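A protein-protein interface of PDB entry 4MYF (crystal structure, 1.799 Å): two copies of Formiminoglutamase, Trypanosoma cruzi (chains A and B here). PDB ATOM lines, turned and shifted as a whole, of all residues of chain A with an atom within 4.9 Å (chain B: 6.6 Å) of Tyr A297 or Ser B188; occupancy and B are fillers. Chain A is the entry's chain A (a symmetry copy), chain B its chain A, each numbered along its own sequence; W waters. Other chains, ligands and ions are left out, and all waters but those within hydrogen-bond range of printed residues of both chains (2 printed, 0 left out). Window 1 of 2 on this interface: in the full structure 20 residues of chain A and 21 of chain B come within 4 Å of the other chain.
The backbone NH (N) of Cys B190 lies within hydrogen-bond range of the side-chain hydroxyl (OG) of Ser A68, at 3.3 Å.
N of Gly B187 is in hydrogen-bond range of OE1 of Glu A73.
N of Ser A68 is in hydrogen-bond range of O of Ser B188 (3.1 Å).
The backbone carbonyl oxygen (O) of Val B254 is in hydrogen-bond range of the side-chain amide nitrogen (NE2) of Gln B186 (2.8 Å).
ND2 of Asn A71 sits at hydrogen-bond distance from OH of Tyr A300.
O of Ser A68 lies within hydrogen-bond range of OH of Tyr A300 (2.4 Å).
The side-chain sulfur of Cys B190 lies within hydrogen-bond range of the backbone carbonyl oxygen of Gln B186 (3.2 Å).
ND1 of His A301 is in hydrogen-bond range of O of Tyr A297, 2.8 Å away.
The side-chain amide oxygen of Asn A71 sits at hydrogen-bond distance from the backbone NH of Glu A73.
Among the printed residues, merely in contact across the chains: Arg A17 with Gln B189 (3.9 Å), Gly A67 with Ser B188 (3.7 Å), Ser A68 with Gly B187 (3.6 Å), Ser A68 with Gln B189 (3.8 Å), Asn A71 with Gly B187 (3.4 Å), Asn A71 with Ser B188 (3.5 Å), Glu A73 with Gln B186 (3.8 Å), Glu A73 with Trp B207 (3.5 Å), Phe A262 with Val B254 (3.6 Å), Arg A293 with Pro B251 (3.96 Å), Val A294 with Ala B253 (3.96 Å), Tyr A297 with Ser B188 (3.8 Å), Tyr A297 with Gln B189 (3.7 Å) and Tyr A300 with Ser B188 (3.5 Å).
Tyr A297 touches just these residues of chain B: Ser B188 and Gln B189.
Of the printed residues of chain A, Gly B187 touches Ser A68 (3.6 Å), Asn A71 (3.4 Å) and Glu A73 (2.8 Å).
Of the printed residues of chain B, Val A294 touches Ala B253 (3.96 Å).
Printed residues of chain A within 4 Å of Gln B186: Glu A73 (3.8 Å).
Printed residues of chain B within 4 Å of Tyr A300: Ser B188 (3.5 Å).
Phe A299 touches none of the printed residues of chain B.
Ala A295 touches none of the printed residues of chain B.
The nearest printed residue of chain A that does not touch Ala B253 is Phe A262 (4.1 Å).
Printed residues of chain B that touch a printed residue of chain A: Gln B186, Gly B187, Ser B188, Gln B189, Cys B190, Trp B207, Pro B251, Ala B253 and Val B254.
Hydrophobic or aromatic side chains of chain B that line the printed part of chain A: Trp B207, Ala B253 and Val B254.
Of the 16 printed residues of chain A, 10 touch a printed residue of chain B.
Hydrophobic or aromatic side chains of chain A within 4 Å of the printed part of chain B: Phe A262, Val A294, Tyr A297 and Tyr A300.
No position is printed for both chains.
Water W1 lies within hydrogen-bond range of the backbone NH of Gly A67, the backbone carbonyl oxygen of Ser B188, the side-chain hydroxyl of Tyr A297 and the guanidinium group of Arg A17.
Water W2 bridges OE1 of Gln B189 and NH2 of Arg A293.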
ATOM      1  N   ARG A  17     -12.983  20.503  16.716  1.00  0.00           N
ATOM      2  CA  ARG A  17     -12.154  19.310  16.833  1.00  0.00           C
ATOM      3  C   ARG A  17     -11.656  18.864  15.471  1.00  0.00           C
ATOM      4  O   ARG A  17     -11.840  19.573  14.492  1.00  0.00           O
ATOM      5  CB  ARG A  17     -12.921  18.201  17.561  1.00  0.00           C
ATOM      6  CG  ARG A  17     -13.297  18.633  18.966  1.00  0.00           C
ATOM      7  CD  ARG A  17     -13.843  17.521  19.825  1.00  0.00           C
ATOM      8  NE  ARG A  17     -13.741  17.879  21.237  1.00  0.00           N
ATOM      9  CZ  ARG A  17     -14.067  17.074  22.244  1.00  0.00           C
ATOM     10  NH1 ARG A  17     -14.525  15.853  21.997  1.00  0.00           N
ATOM     11  NH2 ARG A  17     -13.930  17.489  23.497  1.00  0.00           N
ATOM     12  N   LEU A  66     -13.402  13.470  18.119  1.00  0.00           N
ATOM     13  CA  LEU A  66     -12.352  13.743  19.104  1.00  0.00           C
ATOM     14  C   LEU A  66     -11.342  14.795  18.671  1.00  0.00           C
ATOM     15  O   LEU A  66     -11.206  15.083  17.492  1.00  0.00           O
ATOM     16  CB  LEU A  66     -11.596  12.453  19.440  1.00  0.00           C
ATOM     17  CG  LEU A  66     -12.408  11.250  19.919  1.00  0.00           C
ATOM     18  CD1 LEU A  66     -11.496  10.047  20.158  1.00  0.00           C
ATOM     19  CD2 LEU A  66     -13.190  11.599  21.185  1.00  0.00           C
ATOM     20  N   GLY A  67     -10.647  15.364  19.651  1.00  0.00           N
ATOM     21  CA  GLY A  67      -9.417  16.097  19.403  1.00  0.00           C
ATOM     22  C   GLY A  67      -9.545  17.599  19.241  1.00  0.00           C
ATOM     23  O   GLY A  67      -9.742  18.084  18.129  1.00  0.00           O
ATOM     24  N   SER A  68      -9.388  18.329  20.340  1.00  0.00           N
ATOM     25  CA  SER A  68      -9.423  19.797  20.309  1.00  0.00           C
ATOM     26  C   SER A  68      -8.334  20.362  19.408  1.00  0.00           C
ATOM     27  O   SER A  68      -7.148  20.140  19.644  1.00  0.00           O
ATOM     28  CB  SER A  68      -9.284  20.375  21.720  1.00  0.00           C
ATOM     29  OG  SER A  68     -10.362  19.980  22.546  1.00  0.00           O
ATOM     30  N   ASN A  71      -5.012  23.047  21.290  1.00  0.00           N
ATOM     31  CA  ASN A  71      -4.690  22.352  22.527  1.00  0.00           C
ATOM     32  C   ASN A  71      -3.918  23.284  23.464  1.00  0.00           C
ATOM     33  O   ASN A  71      -2.755  23.598  23.215  1.00  0.00           O
ATOM     34  CB  ASN A  71      -3.851  21.103  22.201  1.00  0.00           C
ATOM     35  CG  ASN A  71      -3.535  20.263  23.431  1.00  0.00           C
ATOM     36  OD1 ASN A  71      -3.175  20.793  24.481  1.00  0.00           O
ATOM     37  ND2 ASN A  71      -3.656  18.938  23.296  1.00  0.00           N
ATOM     38  N   GLU A  73      -3.007  22.714  26.532  1.00  0.00           N
ATOM     39  CA  GLU A  73      -2.050  22.007  27.374  1.00  0.00           C
ATOM     40  C   GLU A  73      -0.683  21.989  26.700  1.00  0.00           C
ATOM     41  O   GLU A  73       0.333  22.329  27.316  1.00  0.00           O
ATOM     42  CB  GLU A  73      -2.517  20.579  27.659  1.00  0.00           C
ATOM     43  CG  GLU A  73      -1.604  19.825  28.616  1.00  0.00           C
ATOM     44  CD  GLU A  73      -2.128  18.436  28.944  1.00  0.00           C
ATOM     45  OE1 GLU A  73      -3.174  18.055  28.395  1.00  0.00           O
ATOM     46  OE2 GLU A  73      -1.492  17.738  29.753  1.00  0.00           O
ATOM     47  N   PHE A 262       1.167   8.682  22.348  1.00  0.00           N
ATOM     48  CA  PHE A 262       0.797  10.066  22.030  1.00  0.00           C
ATOM     49  C   PHE A 262       2.047  10.937  21.865  1.00  0.00           C
ATOM     50  O   PHE A 262       2.168  11.711  20.904  1.00  0.00           O
ATOM     51  CB  PHE A 262      -0.060  10.687  23.147  1.00  0.00           C
ATOM     52  CG  PHE A 262      -1.396  10.027  23.352  1.00  0.00           C
ATOM     53  CD1 PHE A 262      -1.880   9.096  22.444  1.00  0.00           C
ATOM     54  CD2 PHE A 262      -2.174  10.350  24.457  1.00  0.00           C
ATOM     55  CE1 PHE A 262      -3.117   8.489  22.640  1.00  0.00           C
ATOM     56  CE2 PHE A 262      -3.405   9.757  24.659  1.00  0.00           C
ATOM     57  CZ  PHE A 262      -3.881   8.815  23.759  1.00  0.00           C
ATOM     58  N   ARG A 293     -10.416   4.862  20.203  1.00  0.00           N
ATOM     59  CA  ARG A 293     -10.180   6.197  20.748  1.00  0.00           C
ATOM     60  C   ARG A 293      -8.682   6.483  20.901  1.00  0.00           C
ATOM     61  O   ARG A 293      -8.194   7.554  20.507  1.00  0.00           O
ATOM     62  CB  ARG A 293     -10.928   6.377  22.078  1.00  0.00           C
ATOM     63  CG  ARG A 293     -12.455   6.393  21.911  1.00  0.00           C
ATOM     64  CD  ARG A 293     -13.175   6.566  23.256  1.00  0.00           C
ATOM     65  NE  ARG A 293     -12.796   7.827  23.886  1.00  0.00           N
ATOM     66  CZ  ARG A 293     -13.527   8.938  23.855  1.00  0.00           C
ATOM     67  NH1 ARG A 293     -14.708   8.947  23.243  1.00  0.00           N
ATOM     68  NH2 ARG A 293     -13.082  10.037  24.451  1.00  0.00           N
ATOM     69  N   VAL A 294      -7.949   5.531  21.465  1.00  0.00           N
ATOM     70  CA  VAL A 294      -6.495   5.669  21.555  1.00  0.00           C
ATOM     71  C   VAL A 294      -5.883   5.878  20.160  1.00  0.00           C
ATOM     72  O   VAL A 294      -4.981   6.710  19.985  1.00  0.00           O
ATOM     73  CB  VAL A 294      -5.835   4.441  22.216  1.00  0.00           C
ATOM     74  CG1 VAL A 294      -4.299   4.517  22.066  1.00  0.00           C
ATOM     75  CG2 VAL A 294      -6.256   4.338  23.693  1.00  0.00           C
ATOM     76  N   ALA A 295      -6.360   5.119  19.168  1.00  0.00           N
ATOM     77  CA  ALA A 295      -5.841   5.251  17.799  1.00  0.00           C
ATOM     78  C   ALA A 295      -6.070   6.657  17.239  1.00  0.00           C
ATOM     79  O   ALA A 295      -5.176   7.259  16.641  1.00  0.00           O
ATOM     80  CB  ALA A 295      -6.472   4.200  16.862  1.00  0.00           C
ATOM     81  N   VAL A 296      -7.270   7.178  17.434  1.00  0.00           N
ATOM     82  CA  VAL A 296      -7.571   8.527  16.969  1.00  0.00           C
ATOM     83  C   VAL A 296      -6.737   9.572  17.729  1.00  0.00           C
ATOM     84  O   VAL A 296      -6.226  10.509  17.125  1.00  0.00           O
ATOM     85  CB  VAL A 296      -9.087   8.828  17.030  1.00  0.00           C
ATOM     86  CG1 VAL A 296      -9.360  10.310  16.748  1.00  0.00           C
ATOM     87  CG2 VAL A 296      -9.820   7.946  16.019  1.00  0.00           C
ATOM     88  N   TYR A 297      -6.582   9.395  19.043  1.00  0.00           N
ATOM     89  CA  TYR A 297      -5.763  10.310  19.831  1.00  0.00           C
ATOM     90  C   TYR A 297      -4.295  10.273  19.407  1.00  0.00           C
ATOM     91  O   TYR A 297      -3.596  11.278  19.472  1.00  0.00           O
ATOM     92  CB  TYR A 297      -5.907  10.048  21.331  1.00  0.00           C
ATOM     93  CG  TYR A 297      -7.147  10.683  21.938  1.00  0.00           C
ATOM     94  CD1 TYR A 297      -7.418  12.038  21.753  1.00  0.00           C
ATOM     95  CD2 TYR A 297      -8.047   9.935  22.685  1.00  0.00           C
ATOM     96  CE1 TYR A 297      -8.553  12.627  22.299  1.00  0.00           C
ATOM     97  CE2 TYR A 297      -9.181  10.517  23.234  1.00  0.00           C
ATOM     98  CZ  TYR A 297      -9.427  11.865  23.036  1.00  0.00           C
ATOM     99  OH  TYR A 297     -10.545  12.456  23.580  1.00  0.00           O
ATOM    100  N   MET A 298      -3.831   9.114  18.956  1.00  0.00           N
ATOM    101  CA  MET A 298      -2.475   9.009  18.423  1.00  0.00           C
ATOM    102  C   MET A 298      -2.327   9.842  17.155  1.00  0.00           C
ATOM    103  O   MET A 298      -1.361  10.599  16.988  1.00  0.00           O
ATOM    104  CB  MET A 298      -2.118   7.548  18.141  1.00  0.00           C
ATOM    105  CG  MET A 298      -1.713   6.778  19.393  1.00  0.00           C
ATOM    106  SD  MET A 298      -1.600   4.998  19.102  1.00  0.00           S
ATOM    107  CE  MET A 298      -0.155   4.880  18.041  1.00  0.00           C
ATOM    108  N   PHE A 299      -3.277   9.684  16.247  1.00  0.00           N
ATOM    109  CA  PHE A 299      -3.292  10.466  15.001  1.00  0.00           C
ATOM    110  C   PHE A 299      -3.408  11.954  15.320  1.00  0.00           C
ATOM    111  O   PHE A 299      -2.756  12.806  14.701  1.00  0.00           O
ATOM    112  CB  PHE A 299      -4.477  10.028  14.133  1.00  0.00           C
ATOM    113  CG  PHE A 299      -4.727  10.920  12.937  1.00  0.00           C
ATOM    114  CD1 PHE A 299      -3.873  10.892  11.844  1.00  0.00           C
ATOM    115  CD2 PHE A 299      -5.825  11.763  12.906  1.00  0.00           C
ATOM    116  CE1 PHE A 299      -4.100  11.708  10.734  1.00  0.00           C
ATOM    117  CE2 PHE A 299      -6.067  12.583  11.799  1.00  0.00           C
ATOM    118  CZ  PHE A 299      -5.200  12.554  10.714  1.00  0.00           C
ATOM    119  N   TYR A 300      -4.260  12.253  16.294  1.00  0.00           N
ATOM    120  CA  TYR A 300      -4.455  13.619  16.758  1.00  0.00           C
ATOM    121  C   TYR A 300      -3.147  14.268  17.207  1.00  0.00           C
ATOM    122  O   TYR A 300      -2.854  15.407  16.840  1.00  0.00           O
ATOM    123  CB  TYR A 300      -5.461  13.605  17.907  1.00  0.00           C
ATOM    124  CG  TYR A 300      -5.551  14.899  18.693  1.00  0.00           C
ATOM    125  CD1 TYR A 300      -6.130  16.031  18.136  1.00  0.00           C
ATOM    126  CD2 TYR A 300      -5.079  14.977  19.993  1.00  0.00           C
ATOM    127  CE1 TYR A 300      -6.233  17.217  18.854  1.00  0.00           C
ATOM    128  CE2 TYR A 300      -5.171  16.157  20.720  1.00  0.00           C
ATOM    129  CZ  TYR A 300      -5.755  17.271  20.145  1.00  0.00           C
ATOM    130  OH  TYR A 300      -5.857  18.452  20.856  1.00  0.00           O
ATOM    131  N   HIS A 301      -2.358  13.547  18.002  1.00  0.00           N
ATOM    132  CA  HIS A 301      -1.058  14.072  18.424  1.00  0.00           C
ATOM    133  C   HIS A 301      -0.106  14.245  17.239  1.00  0.00           C
ATOM    134  O   HIS A 301       0.654  15.210  17.190  1.00  0.00           O
ATOM    135  CB  HIS A 301      -0.432  13.219  19.546  1.00  0.00           C
ATOM    136  CG  HIS A 301      -1.024  13.491  20.897  1.00  0.00           C
ATOM    137  ND1 HIS A 301      -2.220  12.942  21.306  1.00  0.00           N
ATOM    138  CD2 HIS A 301      -0.614  14.296  21.909  1.00  0.00           C
ATOM    139  CE1 HIS A 301      -2.515  13.381  22.518  1.00  0.00           C
ATOM    140  NE2 HIS A 301      -1.557  14.206  22.906  1.00  0.00           N
ATOM    141  N   GLN B 186      -7.519  17.770  30.502  1.00  0.00           N
ATOM    142  CA  GLN B 186      -6.747  17.289  29.360  1.00  0.00           C
ATOM    143  C   GLN B 186      -6.915  18.181  28.132  1.00  0.00           C
ATOM    144  O   GLN B 186      -8.032  18.429  27.689  1.00  0.00           O
ATOM    145  CB  GLN B 186      -7.103  15.827  29.055  1.00  0.00           C
ATOM    146  CG  GLN B 186      -6.701  14.862  30.188  1.00  0.00           C
ATOM    147  CD  GLN B 186      -7.027  13.402  29.876  1.00  0.00           C
ATOM    148  OE1 GLN B 186      -7.145  13.021  28.717  1.00  0.00           O
ATOM    149  NE2 GLN B 186      -7.166  12.583  30.917  1.00  0.00           N
ATOM    150  N   GLY B 187      -5.791  18.651  27.588  1.00  0.00           N
ATOM    151  CA  GLY B 187      -5.806  19.566  26.461  1.00  0.00           C
ATOM    152  C   GLY B 187      -6.510  19.029  25.231  1.00  0.00           C
ATOM    153  O   GLY B 187      -7.078  19.790  24.454  1.00  0.00           O
ATOM    154  N   SER B 188      -6.480  17.715  25.051  1.00  0.00           N
ATOM    155  CA  SER B 188      -7.132  17.092  23.904  1.00  0.00           C
ATOM    156  C   SER B 188      -8.655  17.154  24.019  1.00  0.00           C
ATOM    157  O   SER B 188      -9.366  16.890  23.046  1.00  0.00           O
ATOM    158  CB  SER B 188      -6.684  15.636  23.781  1.00  0.00           C
ATOM    159  OG  SER B 188      -7.035  14.937  24.956  1.00  0.00           O
ATOM    160  N   GLN B 189      -9.133  17.514  25.211  1.00  0.00           N
ATOM    161  CA  GLN B 189     -10.553  17.499  25.558  1.00  0.00           C
ATOM    162  C   GLN B 189     -11.074  18.832  26.074  1.00  0.00           C
ATOM    163  O   GLN B 189     -12.128  18.867  26.705  1.00  0.00           O
ATOM    164  CB  GLN B 189     -10.803  16.506  26.691  1.00  0.00           C
ATOM    165  CG  GLN B 189     -10.579  15.069  26.352  1.00  0.00           C
ATOM    166  CD  GLN B 189     -11.421  14.194  27.230  1.00  0.00           C
ATOM    167  OE1 GLN B 189     -12.157  13.340  26.742  1.00  0.00           O
ATOM    168  NE2 GLN B 189     -11.365  14.440  28.540  1.00  0.00           N
ATOM    169  N   CYS B 190     -10.350  19.918  25.839  1.00  0.00           N
ATOM    170  CA  CYS B 190     -10.788  21.198  26.366  1.00  0.00           C
ATOM    171  C   CYS B 190     -10.710  22.305  25.305  1.00  0.00           C
ATOM    172  O   CYS B 190      -9.662  22.579  24.726  1.00  0.00           O
ATOM    173  CB  CYS B 190     -10.033  21.524  27.667  1.00  0.00           C
ATOM    174  SG  CYS B 190     -10.262  20.262  29.011  1.00  0.00           S
ATOM    175  N   TRP B 207      -3.158  21.166  34.220  1.00  0.00           N
ATOM    176  CA  TRP B 207      -3.251  20.112  33.202  1.00  0.00           C
ATOM    177  C   TRP B 207      -2.683  18.781  33.694  1.00  0.00           C
ATOM    178  O   TRP B 207      -1.781  18.763  34.532  1.00  0.00           O
ATOM    179  CB  TRP B 207      -2.483  20.535  31.947  1.00  0.00           C
ATOM    180  CG  TRP B 207      -3.006  21.778  31.300  1.00  0.00           C
ATOM    181  CD1 TRP B 207      -2.438  23.027  31.328  1.00  0.00           C
ATOM    182  CD2 TRP B 207      -4.205  21.898  30.525  1.00  0.00           C
ATOM    183  NE1 TRP B 207      -3.216  23.914  30.616  1.00  0.00           N
ATOM    184  CE2 TRP B 207      -4.306  23.246  30.115  1.00  0.00           C
ATOM    185  CE3 TRP B 207      -5.209  20.998  30.144  1.00  0.00           C
ATOM    186  CZ2 TRP B 207      -5.363  23.709  29.335  1.00  0.00           C
ATOM    187  CZ3 TRP B 207      -6.261  21.466  29.358  1.00  0.00           C
ATOM    188  CH2 TRP B 207      -6.331  22.808  28.971  1.00  0.00           C
ATOM    189  N   PRO B 251     -14.999   7.272  29.217  1.00  0.00           N
ATOM    190  CA  PRO B 251     -13.714   6.644  29.577  1.00  0.00           C
ATOM    191  C   PRO B 251     -12.482   7.363  29.016  1.00  0.00           C
ATOM    192  O   PRO B 251     -12.447   7.730  27.828  1.00  0.00           O
ATOM    193  CB  PRO B 251     -13.841   5.226  28.999  1.00  0.00           C
ATOM    194  CG  PRO B 251     -15.342   4.980  28.955  1.00  0.00           C
ATOM    195  CD  PRO B 251     -15.926   6.318  28.580  1.00  0.00           C
ATOM    196  N   ALA B 252     -11.482   7.568  29.874  1.00  0.00           N
ATOM    197  CA  ALA B 252     -10.296   8.333  29.493  1.00  0.00           C
ATOM    198  C   ALA B 252      -9.187   7.424  28.974  1.00  0.00           C
ATOM    199  O   ALA B 252      -8.936   6.375  29.543  1.00  0.00           O
ATOM    200  CB  ALA B 252      -9.789   9.165  30.666  1.00  0.00           C
ATOM    201  N   ALA B 253      -8.528   7.830  27.890  1.00  0.00           N
ATOM    202  CA  ALA B 253      -7.412   7.044  27.355  1.00  0.00           C
ATOM    203  C   ALA B 253      -6.191   7.160  28.276  1.00  0.00           C
ATOM    204  O   ALA B 253      -5.544   6.156  28.619  1.00  0.00           O
ATOM    205  CB  ALA B 253      -7.071   7.501  25.939  1.00  0.00           C
ATOM    206  N   VAL B 254      -5.891   8.395  28.671  1.00  0.00           N
ATOM    207  CA  VAL B 254      -4.891   8.678  29.694  1.00  0.00           C
ATOM    208  C   VAL B 254      -5.559   9.394  30.880  1.00  0.00           C
ATOM    209  O   VAL B 254      -6.682   9.868  30.772  1.00  0.00           O
ATOM    210  CB  VAL B 254      -3.736   9.549  29.149  1.00  0.00           C
ATOM    211  CG1 VAL B 254      -2.900   8.765  28.120  1.00  0.00           C
ATOM    212  CG2 VAL B 254      -4.279  10.844  28.543  1.00  0.00           C
HETATM  213  O   HOH W   1     -11.247  14.921  22.343  1.00  0.00           O
HETATM  214  O   HOH W   2     -14.692  11.916  26.875  1.00  0.00           O
